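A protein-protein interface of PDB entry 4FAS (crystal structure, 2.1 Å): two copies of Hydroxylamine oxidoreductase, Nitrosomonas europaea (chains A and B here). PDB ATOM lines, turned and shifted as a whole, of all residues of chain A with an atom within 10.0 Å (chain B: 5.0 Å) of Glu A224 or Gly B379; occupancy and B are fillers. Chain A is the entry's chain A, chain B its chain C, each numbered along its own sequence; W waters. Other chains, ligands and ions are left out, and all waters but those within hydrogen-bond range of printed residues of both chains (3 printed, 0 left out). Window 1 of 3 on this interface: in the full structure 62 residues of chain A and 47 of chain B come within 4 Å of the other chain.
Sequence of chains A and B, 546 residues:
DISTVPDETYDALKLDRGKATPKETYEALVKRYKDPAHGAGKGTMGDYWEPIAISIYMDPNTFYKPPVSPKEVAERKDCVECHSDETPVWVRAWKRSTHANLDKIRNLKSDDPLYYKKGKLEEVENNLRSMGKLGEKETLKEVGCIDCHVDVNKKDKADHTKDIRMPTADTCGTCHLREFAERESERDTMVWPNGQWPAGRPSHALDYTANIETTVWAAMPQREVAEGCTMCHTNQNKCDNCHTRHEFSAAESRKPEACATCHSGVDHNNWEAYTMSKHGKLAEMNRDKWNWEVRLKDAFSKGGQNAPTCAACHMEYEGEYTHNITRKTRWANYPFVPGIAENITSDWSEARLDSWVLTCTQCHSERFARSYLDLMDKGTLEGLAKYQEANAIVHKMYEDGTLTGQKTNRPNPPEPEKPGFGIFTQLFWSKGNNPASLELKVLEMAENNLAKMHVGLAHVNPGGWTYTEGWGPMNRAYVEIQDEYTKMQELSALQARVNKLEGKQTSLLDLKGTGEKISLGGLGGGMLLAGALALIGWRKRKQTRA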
ATOM      1  N   TRP A  49      18.300 -26.453  28.534  1.00  0.00           N
ATOM      2  CA  TRP A  49      16.953 -25.917  28.363  1.00  0.00           C
ATOM      3  C   TRP A  49      16.028 -26.941  27.735  1.00  0.00           C
ATOM      4  O   TRP A  49      16.492 -27.868  27.144  1.00  0.00           O
ATOM      5  CB  TRP A  49      17.010 -24.652  27.503  1.00  0.00           C
ATOM      6  CG  TRP A  49      17.648 -24.909  26.098  1.00  0.00           C
ATOM      7  CD1 TRP A  49      18.954 -24.938  25.786  1.00  0.00           C
ATOM      8  CD2 TRP A  49      16.931 -25.155  24.888  1.00  0.00           C
ATOM      9  NE1 TRP A  49      19.122 -25.165  24.416  1.00  0.00           N
ATOM     10  CE2 TRP A  49      17.883 -25.358  23.862  1.00  0.00           C
ATOM     11  CE3 TRP A  49      15.566 -25.221  24.570  1.00  0.00           C
ATOM     12  CZ2 TRP A  49      17.515 -25.598  22.527  1.00  0.00           C
ATOM     13  CZ3 TRP A  49      15.187 -25.486  23.220  1.00  0.00           C
ATOM     14  CH2 TRP A  49      16.168 -25.638  22.228  1.00  0.00           C
ATOM     15  N   GLU A  50      14.711 -26.743  27.934  1.00  0.00           N
ATOM     16  CA  GLU A  50      13.672 -27.510  27.311  1.00  0.00           C
ATOM     17  C   GLU A  50      12.674 -26.554  26.560  1.00  0.00           C
ATOM     18  O   GLU A  50      12.481 -25.407  26.951  1.00  0.00           O
ATOM     19  CB  GLU A  50      12.917 -28.292  28.389  1.00  0.00           C
ATOM     20  CG  GLU A  50      13.723 -29.356  29.102  1.00  0.00           C
ATOM     21  CD  GLU A  50      14.808 -28.794  30.044  1.00  0.00           C
ATOM     22  OE1 GLU A  50      14.475 -28.100  31.051  1.00  0.00           O
ATOM     23  OE2 GLU A  50      16.023 -29.039  29.778  1.00  0.00           O
ATOM     24  N   PRO A  51      12.021 -27.066  25.519  1.00  0.00           N
ATOM     25  CA  PRO A  51      11.112 -26.312  24.766  1.00  0.00           C
ATOM     26  C   PRO A  51       9.926 -25.933  25.655  1.00  0.00           C
ATOM     27  O   PRO A  51       9.646 -26.656  26.602  1.00  0.00           O
ATOM     28  CB  PRO A  51      10.706 -27.299  23.639  1.00  0.00           C
ATOM     29  CG  PRO A  51      10.865 -28.682  24.271  1.00  0.00           C
ATOM     30  CD  PRO A  51      12.121 -28.467  25.041  1.00  0.00           C
ATOM     31  N   ILE A  52       9.290 -24.783  25.365  1.00  0.00           N
ATOM     32  CA  ILE A  52       7.934 -24.460  25.857  1.00  0.00           C
ATOM     33  C   ILE A  52       6.921 -24.674  24.713  1.00  0.00           C
ATOM     34  O   ILE A  52       7.319 -24.991  23.582  1.00  0.00           O
ATOM     35  CB  ILE A  52       7.843 -23.013  26.387  1.00  0.00           C
ATOM     36  CG1 ILE A  52       8.073 -21.991  25.255  1.00  0.00           C
ATOM     37  CG2 ILE A  52       8.833 -22.822  27.574  1.00  0.00           C
ATOM     38  CD1 ILE A  52       8.097 -20.487  25.772  1.00  0.00           C
ATOM     39  N   ALA A  53       5.632 -24.494  24.969  1.00  0.00           N
ATOM     40  CA  ALA A  53       4.611 -24.893  23.996  1.00  0.00           C
ATOM     41  C   ALA A  53       4.812 -24.287  22.610  1.00  0.00           C
ATOM     42  O   ALA A  53       4.705 -24.996  21.611  1.00  0.00           O
ATOM     43  CB  ALA A  53       3.194 -24.589  24.508  1.00  0.00           C
ATOM     44  N   ILE A  54       5.097 -22.982  22.552  1.00  0.00           N
ATOM     45  CA  ILE A  54       5.325 -22.286  21.258  1.00  0.00           C
ATOM     46  C   ILE A  54       6.575 -22.769  20.468  1.00  0.00           C
ATOM     47  O   ILE A  54       6.653 -22.530  19.253  1.00  0.00           O
ATOM     48  CB  ILE A  54       5.360 -20.733  21.406  1.00  0.00           C
ATOM     49  CG1 ILE A  54       5.058 -20.022  20.069  1.00  0.00           C
ATOM     50  CG2 ILE A  54       6.750 -20.276  21.799  1.00  0.00           C
ATOM     51  CD1 ILE A  54       3.588 -19.627  19.786  1.00  0.00           C
ATOM     52  N   SER A  55       7.549 -23.421  21.106  1.00  0.00           N
ATOM     53  CA  SER A  55       8.782 -23.837  20.367  1.00  0.00           C
ATOM     54  C   SER A  55       8.538 -24.813  19.275  1.00  0.00           C
ATOM     55  O   SER A  55       9.370 -24.957  18.373  1.00  0.00           O
ATOM     56  CB  SER A  55       9.764 -24.511  21.315  1.00  0.00           C
ATOM     57  OG  SER A  55       9.882 -23.716  22.467  1.00  0.00           O
ATOM     58  N   MET A  58       8.571 -22.645  16.498  1.00  0.00           N
ATOM     59  CA  MET A  58       9.845 -21.896  16.338  1.00  0.00           C
ATOM     60  C   MET A  58      10.939 -22.729  15.764  1.00  0.00           C
ATOM     61  O   MET A  58      11.729 -22.204  14.958  1.00  0.00           O
ATOM     62  CB  MET A  58      10.373 -21.281  17.649  1.00  0.00           C
ATOM     63  CG  MET A  58       9.229 -20.531  18.420  1.00  0.00           C
ATOM     64  SD  MET A  58       8.974 -18.851  17.749  1.00  0.00           S
ATOM     65  CE  MET A  58       7.823 -18.971  16.425  1.00  0.00           C
ATOM     66  N   TRP A 217      20.579 -17.124  26.962  1.00  0.00           N
ATOM     67  CA  TRP A 217      19.353 -17.690  26.434  1.00  0.00           C
ATOM     68  C   TRP A 217      19.166 -19.142  26.844  1.00  0.00           C
ATOM     69  O   TRP A 217      17.981 -19.554  27.088  1.00  0.00           O
ATOM     70  CB  TRP A 217      19.334 -17.667  24.900  1.00  0.00           C
ATOM     71  CG  TRP A 217      18.043 -18.200  24.341  1.00  0.00           C
ATOM     72  CD1 TRP A 217      16.883 -17.490  24.088  1.00  0.00           C
ATOM     73  CD2 TRP A 217      17.761 -19.560  24.005  1.00  0.00           C
ATOM     74  NE1 TRP A 217      15.906 -18.324  23.568  1.00  0.00           N
ATOM     75  CE2 TRP A 217      16.425 -19.597  23.493  1.00  0.00           C
ATOM     76  CE3 TRP A 217      18.518 -20.749  24.048  1.00  0.00           C
ATOM     77  CZ2 TRP A 217      15.807 -20.794  23.105  1.00  0.00           C
ATOM     78  CZ3 TRP A 217      17.920 -21.920  23.622  1.00  0.00           C
ATOM     79  CH2 TRP A 217      16.570 -21.935  23.158  1.00  0.00           C
ATOM     80  N   MET A 220      19.153 -18.993  31.372  1.00  0.00           N
ATOM     81  CA  MET A 220      18.228 -18.261  32.252  1.00  0.00           C
ATOM     82  C   MET A 220      16.940 -19.044  32.538  1.00  0.00           C
ATOM     83  O   MET A 220      16.484 -19.832  31.730  1.00  0.00           O
ATOM     84  CB  MET A 220      17.854 -16.875  31.689  1.00  0.00           C
ATOM     85  CG  MET A 220      17.052 -16.960  30.386  1.00  0.00           C
ATOM     86  SD  MET A 220      17.071 -15.367  29.488  1.00  0.00           S
ATOM     87  CE  MET A 220      15.896 -14.459  30.507  1.00  0.00           C
ATOM     88  N   PRO A 221      16.356 -18.820  33.692  1.00  0.00           N
ATOM     89  CA  PRO A 221      15.170 -19.603  33.971  1.00  0.00           C
ATOM     90  C   PRO A 221      13.887 -18.997  33.395  1.00  0.00           C
ATOM     91  O   PRO A 221      12.898 -19.695  33.360  1.00  0.00           O
ATOM     92  CB  PRO A 221      15.108 -19.612  35.521  1.00  0.00           C
ATOM     93  CG  PRO A 221      15.743 -18.397  35.914  1.00  0.00           C
ATOM     94  CD  PRO A 221      16.883 -18.167  34.897  1.00  0.00           C
ATOM     95  N   GLN A 222      13.885 -17.718  32.946  1.00  0.00           N
ATOM     96  CA  GLN A 222      12.634 -17.123  32.474  1.00  0.00           C
ATOM     97  C   GLN A 222      12.393 -17.523  31.051  1.00  0.00           C
ATOM     98  O   GLN A 222      12.654 -16.733  30.150  1.00  0.00           O
ATOM     99  CB  GLN A 222      12.642 -15.607  32.566  1.00  0.00           C
ATOM    100  CG  GLN A 222      12.749 -15.069  33.958  1.00  0.00           C
ATOM    101  CD  GLN A 222      14.175 -15.134  34.497  1.00  0.00           C
ATOM    102  OE1 GLN A 222      15.120 -15.528  33.797  1.00  0.00           O
ATOM    103  NE2 GLN A 222      14.326 -14.768  35.749  1.00  0.00           N
ATOM    104  N   ARG A 223      11.883 -18.730  30.834  1.00  0.00           N
ATOM    105  CA  ARG A 223      11.819 -19.271  29.453  1.00  0.00           C
ATOM    106  C   ARG A 223      11.007 -18.377  28.502  1.00  0.00           C
ATOM    107  O   ARG A 223      11.341 -18.229  27.337  1.00  0.00           O
ATOM    108  CB  ARG A 223      11.261 -20.725  29.395  1.00  0.00           C
ATOM    109  CG  ARG A 223      12.170 -21.743  30.052  1.00  0.00           C
ATOM    110  CD  ARG A 223      13.660 -21.388  29.833  1.00  0.00           C
ATOM    111  NE  ARG A 223      14.095 -21.608  28.469  1.00  0.00           N
ATOM    112  CZ  ARG A 223      15.253 -21.131  28.025  1.00  0.00           C
ATOM    113  NH1 ARG A 223      16.056 -20.455  28.869  1.00  0.00           N
ATOM    114  NH2 ARG A 223      15.579 -21.277  26.764  1.00  0.00           N
ATOM    115  N   GLU A 224       9.931 -17.799  29.005  1.00  0.00           N
ATOM    116  CA  GLU A 224       9.019 -16.987  28.166  1.00  0.00           C
ATOM    117  C   GLU A 224       9.659 -15.658  27.726  1.00  0.00           C
ATOM    118  O   GLU A 224       9.413 -15.184  26.602  1.00  0.00           O
ATOM    119  CB  GLU A 224       7.672 -16.796  28.911  1.00  0.00           C
ATOM    120  CG  GLU A 224       6.756 -18.072  28.835  1.00  0.00           C
ATOM    121  CD  GLU A 224       7.264 -19.309  29.681  1.00  0.00           C
ATOM    122  OE1 GLU A 224       8.086 -19.151  30.660  1.00  0.00           O
ATOM    123  OE2 GLU A 224       6.785 -20.436  29.367  1.00  0.00           O
ATOM    124  N   VAL A 225      10.526 -15.097  28.570  1.00  0.00           N
ATOM    125  CA  VAL A 225      11.387 -13.995  28.183  1.00  0.00           C
ATOM    126  C   VAL A 225      12.340 -14.439  27.106  1.00  0.00           C
ATOM    127  O   VAL A 225      12.438 -13.810  26.032  1.00  0.00           O
ATOM    128  CB  VAL A 225      12.144 -13.393  29.427  1.00  0.00           C
ATOM    129  CG1 VAL A 225      13.212 -12.328  29.057  1.00  0.00           C
ATOM    130  CG2 VAL A 225      11.165 -12.842  30.399  1.00  0.00           C
ATOM    131  N   ALA A 226      13.023 -15.547  27.328  1.00  0.00           N
ATOM    132  CA  ALA A 226      14.009 -15.997  26.362  1.00  0.00           C
ATOM    133  C   ALA A 226      13.374 -16.306  24.983  1.00  0.00           C
ATOM    134  O   ALA A 226      14.004 -16.090  23.913  1.00  0.00           O
ATOM    135  CB  ALA A 226      14.787 -17.246  26.936  1.00  0.00           C
ATOM    136  N   GLU A 227      12.160 -16.839  24.994  1.00  0.00           N
ATOM    137  CA  GLU A 227      11.460 -17.174  23.745  1.00  0.00           C
ATOM    138  C   GLU A 227      11.023 -15.925  22.928  1.00  0.00           C
ATOM    139  O   GLU A 227      10.785 -16.031  21.730  1.00  0.00           O
ATOM    140  CB  GLU A 227      10.263 -18.042  24.013  1.00  0.00           C
ATOM    141  CG  GLU A 227      10.134 -19.208  23.046  1.00  0.00           C
ATOM    142  CD  GLU A 227      11.319 -20.143  23.255  1.00  0.00           C
ATOM    143  OE1 GLU A 227      11.526 -20.644  24.414  1.00  0.00           O
ATOM    144  OE2 GLU A 227      12.121 -20.274  22.318  1.00  0.00           O
ATOM    145  N   GLY A 228      11.015 -14.739  23.521  1.00  0.00           N
ATOM    146  CA  GLY A 228      10.857 -13.508  22.707  1.00  0.00           C
ATOM    147  C   GLY A 228      12.121 -13.308  21.929  1.00  0.00           C
ATOM    148  O   GLY A 228      12.111 -12.786  20.798  1.00  0.00           O
ATOM    149  N   CYS A 229      13.270 -13.663  22.488  1.00  0.00           N
ATOM    150  CA  CYS A 229      14.463 -13.675  21.611  1.00  0.00           C
ATOM    151  C   CYS A 229      14.318 -14.643  20.479  1.00  0.00           C
ATOM    152  O   CYS A 229      14.615 -14.285  19.353  1.00  0.00           O
ATOM    153  CB  CYS A 229      15.745 -13.992  22.343  1.00  0.00           C
ATOM    154  SG  CYS A 229      15.885 -12.927  23.775  1.00  0.00           S
ATOM    155  N   THR A 230      13.821 -15.836  20.738  1.00  0.00           N
ATOM    156  CA  THR A 230      13.671 -16.839  19.651  1.00  0.00           C
ATOM    157  C   THR A 230      12.749 -16.303  18.537  1.00  0.00           C
ATOM    158  O   THR A 230      13.034 -16.482  17.349  1.00  0.00           O
ATOM    159  CB  THR A 230      13.075 -18.077  20.214  1.00  0.00           C
ATOM    160  OG1 THR A 230      13.932 -18.525  21.290  1.00  0.00           O
ATOM    161  CG2 THR A 230      12.824 -19.135  19.071  1.00  0.00           C
ATOM    162  N   MET A 231      11.697 -15.562  18.917  1.00  0.00           N
ATOM    163  CA  MET A 231      10.783 -15.003  17.914  1.00  0.00           C
ATOM    164  C   MET A 231      11.440 -14.128  16.852  1.00  0.00           C
ATOM    165  O   MET A 231      10.995 -14.076  15.710  1.00  0.00           O
ATOM    166  CB  MET A 231       9.528 -14.326  18.545  1.00  0.00           C
ATOM    167  CG  MET A 231       8.586 -15.372  19.176  1.00  0.00           C
ATOM    168  SD  MET A 231       7.115 -14.608  19.974  1.00  0.00           S
ATOM    169  CE  MET A 231       6.389 -13.980  18.487  1.00  0.00           C
ATOM    170  N   PHE A 428      20.499  -9.922  30.622  1.00  0.00           N
ATOM    171  CA  PHE A 428      19.309 -10.764  30.806  1.00  0.00           C
ATOM    172  C   PHE A 428      19.175 -11.456  32.183  1.00  0.00           C
ATOM    173  O   PHE A 428      18.129 -12.055  32.518  1.00  0.00           O
ATOM    174  CB  PHE A 428      19.143 -11.754  29.629  1.00  0.00           C
ATOM    175  CG  PHE A 428      18.573 -11.100  28.422  1.00  0.00           C
ATOM    176  CD1 PHE A 428      17.188 -11.115  28.207  1.00  0.00           C
ATOM    177  CD2 PHE A 428      19.415 -10.345  27.565  1.00  0.00           C
ATOM    178  CE1 PHE A 428      16.622 -10.434  27.083  1.00  0.00           C
ATOM    179  CE2 PHE A 428      18.914  -9.645  26.474  1.00  0.00           C
ATOM    180  CZ  PHE A 428      17.478  -9.693  26.235  1.00  0.00           C
ATOM    181  N   ASP B 374      -0.267 -18.808  26.632  1.00  0.00           N
ATOM    182  CA  ASP B 374       0.477 -19.381  27.760  1.00  0.00           C
ATOM    183  C   ASP B 374       1.817 -18.639  28.016  1.00  0.00           C
ATOM    184  O   ASP B 374       2.147 -18.234  29.167  1.00  0.00           O
ATOM    185  CB  ASP B 374       0.731 -20.829  27.527  1.00  0.00           C
ATOM    186  CG  ASP B 374       1.294 -21.507  28.780  1.00  0.00           C
ATOM    187  OD1 ASP B 374       2.496 -21.873  28.789  1.00  0.00           O
ATOM    188  OD2 ASP B 374       0.548 -21.612  29.771  1.00  0.00           O
ATOM    189  N   LEU B 375       2.564 -18.429  26.935  1.00  0.00           N
ATOM    190  CA  LEU B 375       3.728 -17.565  26.983  1.00  0.00           C
ATOM    191  C   LEU B 375       3.393 -16.148  27.577  1.00  0.00           C
ATOM    192  O   LEU B 375       4.105 -15.638  28.466  1.00  0.00           O
ATOM    193  CB  LEU B 375       4.347 -17.506  25.600  1.00  0.00           C
ATOM    194  CG  LEU B 375       5.620 -16.733  25.350  1.00  0.00           C
ATOM    195  CD1 LEU B 375       6.308 -17.180  23.987  1.00  0.00           C
ATOM    196  CD2 LEU B 375       5.328 -15.243  25.376  1.00  0.00           C
ATOM    197  N   MET B 376       2.304 -15.534  27.133  1.00  0.00           N
ATOM    198  CA  MET B 376       1.964 -14.214  27.623  1.00  0.00           C
ATOM    199  C   MET B 376       1.757 -14.278  29.127  1.00  0.00           C
ATOM    200  O   MET B 376       2.230 -13.384  29.876  1.00  0.00           O
ATOM    201  CB  MET B 376       0.654 -13.692  26.972  1.00  0.00           C
ATOM    202  CG  MET B 376       0.093 -12.463  27.697  1.00  0.00           C
ATOM    203  SD  MET B 376      -1.535 -12.060  27.039  1.00  0.00           S
ATOM    204  CE  MET B 376      -2.597 -13.321  27.766  1.00  0.00           C
ATOM    205  N   ASP B 377       0.939 -15.238  29.590  1.00  0.00           N
ATOM    206  CA  ASP B 377       0.662 -15.267  31.033  1.00  0.00           C
ATOM    207  C   ASP B 377       1.905 -15.517  31.923  1.00  0.00           C
ATOM    208  O   ASP B 377       2.092 -14.830  32.948  1.00  0.00           O
ATOM    209  CB  ASP B 377      -0.447 -16.295  31.405  1.00  0.00           C
ATOM    210  CG  ASP B 377      -1.836 -15.879  30.924  1.00  0.00           C
ATOM    211  OD1 ASP B 377      -2.120 -14.643  30.698  1.00  0.00           O
ATOM    212  OD2 ASP B 377      -2.696 -16.823  30.842  1.00  0.00           O
ATOM    213  N   LYS B 378       2.739 -16.477  31.541  1.00  0.00           N
ATOM    214  CA  LYS B 378       3.957 -16.789  32.315  1.00  0.00           C
ATOM    215  C   LYS B 378       5.051 -15.752  32.187  1.00  0.00           C
ATOM    216  O   LYS B 378       5.752 -15.441  33.199  1.00  0.00           O
ATOM    217  CB  LYS B 378       4.512 -18.182  31.920  1.00  0.00           C
ATOM    218  CG  LYS B 378       3.481 -19.277  32.090  1.00  0.00           C
ATOM    219  CD  LYS B 378       4.067 -20.657  31.892  1.00  0.00           C
ATOM    220  CE  LYS B 378       3.036 -21.657  32.277  1.00  0.00           C
ATOM    221  NZ  LYS B 378       3.506 -22.932  31.660  1.00  0.00           N
ATOM    222  N   GLY B 379       5.251 -15.207  30.975  1.00  0.00           N
ATOM    223  CA  GLY B 379       6.181 -14.057  30.859  1.00  0.00           C
ATOM    224  C   GLY B 379       5.741 -12.843  31.742  1.00  0.00           C
ATOM    225  O   GLY B 379       6.580 -12.213  32.450  1.00  0.00           O
ATOM    226  N   THR B 380       4.418 -12.535  31.768  1.00  0.00           N
ATOM    227  CA  THR B 380       3.928 -11.471  32.654  1.00  0.00           C
ATOM    228  C   THR B 380       4.370 -11.720  34.134  1.00  0.00           C
ATOM    229  O   THR B 380       5.012 -10.862  34.837  1.00  0.00           O
ATOM    230  CB  THR B 380       2.407 -11.267  32.462  1.00  0.00           C
ATOM    231  OG1 THR B 380       2.179 -10.843  31.110  1.00  0.00           O
ATOM    232  CG2 THR B 380       1.824 -10.184  33.398  1.00  0.00           C
ATOM    233  N   LEU B 381       4.125 -12.951  34.565  1.00  0.00           N
ATOM    234  CA  LEU B 381       4.445 -13.356  35.922  1.00  0.00           C
ATOM    235  C   LEU B 381       5.954 -13.353  36.162  1.00  0.00           C
ATOM    236  O   LEU B 381       6.402 -13.025  37.281  1.00  0.00           O
ATOM    237  CB  LEU B 381       3.834 -14.770  36.182  1.00  0.00           C
ATOM    238  CG  LEU B 381       2.354 -14.984  36.438  1.00  0.00           C
ATOM    239  CD1 LEU B 381       1.903 -16.449  36.454  1.00  0.00           C
ATOM    240  CD2 LEU B 381       1.885 -14.272  37.698  1.00  0.00           C
ATOM    241  N   GLU B 382       6.765 -13.736  35.162  1.00  0.00           N
ATOM    242  CA  GLU B 382       8.252 -13.555  35.297  1.00  0.00           C
ATOM    243  C   GLU B 382       8.705 -12.136  35.545  1.00  0.00           C
ATOM    244  O   GLU B 382       9.578 -11.885  36.343  1.00  0.00           O
ATOM    245  CB  GLU B 382       9.013 -14.161  34.113  1.00  0.00           C
ATOM    246  CG  GLU B 382       8.892 -15.747  34.129  1.00  0.00           C
ATOM    247  CD  GLU B 382       8.848 -16.416  32.717  1.00  0.00           C
ATOM    248  OE1 GLU B 382       9.329 -15.816  31.743  1.00  0.00           O
ATOM    249  OE2 GLU B 382       8.390 -17.584  32.633  1.00  0.00           O
ATOM    250  N   GLY B 383       8.113 -11.184  34.838  1.00  0.00           N
ATOM    251  CA  GLY B 383       8.320  -9.784  35.110  1.00  0.00           C
ATOM    252  C   GLY B 383       7.843  -9.420  36.504  1.00  0.00           C
ATOM    253  O   GLY B 383       8.592  -8.791  37.258  1.00  0.00           O
ATOM    254  N   MET B 453       6.126  -4.408  29.889  1.00  0.00           N
ATOM    255  CA  MET B 453       6.481  -5.789  29.574  1.00  0.00           C
ATOM    256  C   MET B 453       5.203  -6.613  29.294  1.00  0.00           C
ATOM    257  O   MET B 453       5.145  -7.413  28.308  1.00  0.00           O
ATOM    258  CB  MET B 453       7.241  -6.405  30.729  1.00  0.00           C
ATOM    259  CG  MET B 453       7.802  -7.768  30.397  1.00  0.00           C
ATOM    260  SD  MET B 453       8.610  -8.527  31.818  1.00  0.00           S
ATOM    261  CE  MET B 453       9.051 -10.121  30.996  1.00  0.00           C
ATOM    262  N   LEU B 457       3.996  -8.392  25.677  1.00  0.00           N
ATOM    263  CA  LEU B 457       3.562  -9.781  25.633  1.00  0.00           C
ATOM    264  C   LEU B 457       2.171  -9.919  25.053  1.00  0.00           C
ATOM    265  O   LEU B 457       1.971 -10.815  24.136  1.00  0.00           O
ATOM    266  CB  LEU B 457       3.604 -10.461  27.003  1.00  0.00           C
ATOM    267  CG  LEU B 457       5.047 -10.722  27.453  1.00  0.00           C
ATOM    268  CD1 LEU B 457       5.191 -10.582  28.910  1.00  0.00           C
ATOM    269  CD2 LEU B 457       5.584 -12.095  26.945  1.00  0.00           C
ATOM    270  N   TRP B 465       9.084  -6.986  25.272  1.00  0.00           N
ATOM    271  CA  TRP B 465       9.145  -7.627  26.581  1.00  0.00           C
ATOM    272  C   TRP B 465      10.588  -8.137  26.927  1.00  0.00           C
ATOM    273  O   TRP B 465      10.810  -8.604  28.068  1.00  0.00           O
ATOM    274  CB  TRP B 465       8.086  -8.718  26.737  1.00  0.00           C
ATOM    275  CG  TRP B 465       8.342 -10.083  26.091  1.00  0.00           C
ATOM    276  CD1 TRP B 465       9.119 -11.110  26.561  1.00  0.00           C
ATOM    277  CD2 TRP B 465       7.710 -10.596  24.867  1.00  0.00           C
ATOM    278  NE1 TRP B 465       8.966 -12.231  25.740  1.00  0.00           N
ATOM    279  CE2 TRP B 465       8.124 -11.924  24.696  1.00  0.00           C
ATOM    280  CE3 TRP B 465       6.808 -10.042  23.949  1.00  0.00           C
ATOM    281  CZ2 TRP B 465       7.699 -12.724  23.597  1.00  0.00           C
ATOM    282  CZ3 TRP B 465       6.345 -10.839  22.854  1.00  0.00           C
ATOM    283  CH2 TRP B 465       6.795 -12.162  22.687  1.00  0.00           C
HETATM  284  O   HOH W   1       4.936 -21.127  27.750  1.00  0.00           O
HETATM  285  O   HOH W   2       4.691 -23.930  27.472  1.00  0.00           O
HETATM  286  O   HOH W   3      11.797 -13.374  37.156  1.00  0.00           O
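Water W1 bridges the side-chain carboxylate (OE2) of Glu A224 and the side-chain carboxylate (OD1) of Asp B374.
Water W2 bridges N of Ala A53 (2.7 Å) and OD1 of Asp B374 (3.3 Å).
Water W3 lies within hydrogen-bond range of O of Glu B382 and NE2 of Gln A222.
Among the printed residues, pairs that only touch across the chains: Gly A228 with Trp B465, Gln A222 with Glu B382, Val A225 with Met B453, Glu A224 with Gly B379, Glu A224 with Leu B375, Met A231 with Trp B465, Glu A224 with Lys B378, Ile A54 with Leu B375, Val A225 with Trp B465 and Arg A223 with Glu B382.
Printed residues of chain B that touch a printed residue of chain A: Leu B375, Lys B378, Gly B379, Glu B382, Met B453 and Trp B465.
Among the printed residues, 13 pairs touch across the chains.
Among the printed residues, no Asp or Glu carboxylate lies within 4 Å of a Lys or Arg side-chain nitrogen of the other chain.
The backbone NH of Glu A224 lies close to the side-chain carboxylate of Glu B382, 3.4 Å away.
The indole nitrogen (NE1) of Trp B465 lies within hydrogen-bond range of the backbone carbonyl oxygen (O) of Glu A224 (3.1 Å).
The backbone NH of Val A225 is in hydrogen-bond range of the side-chain carboxylate of Glu B382 (3.5 Å).
No position is printed for both chains.
Glu A224 touches five residues of chain B.
Of chain A, only Glu A224 comes within 4 Å of Gly B379.
Of the printed residues of chain A, Leu B375 touches Ile A54 (3.8 Å) and Glu A224 (3.6 Å).
Lys B378 touches just one residue of chain A: Glu A224.
No residue of chain A comes within 4 Å of Thr B380.
Printed residues of chain B within 4 Å of Gly A228: Trp B465 (3.4 Å).
Of the printed residues of chain B, Ile A54 touches Leu B375.
Of the printed residues of chain A, Trp B465 touches Glu A224 (3.1 Å), Val A225 (3.8 Å), Gly A228 (3.4 Å) and Met A231 (3.7 Å).
Of the printed residues of chain B, Arg A223 touches Glu B382 (3.98 Å).
Of the printed residues of chain B, Met A231 touches Trp B465.
Ser A55 touches none of the printed residues of chain B.
The nearest residue of chain A that does not touch Gly B379 is Val A225 (5.0 Å).
O of Trp A217 sits at hydrogen-bond distance from NH1 of Arg A223.
O of Met A220 is in hydrogen-bond range of NH1 of Arg A223, at 3.0 Å.
The side-chain amino group (NZ) of Lys B378 is in salt-bridge range of the side-chain carboxylate (OD1) of Asp B374 (3.2 Å).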
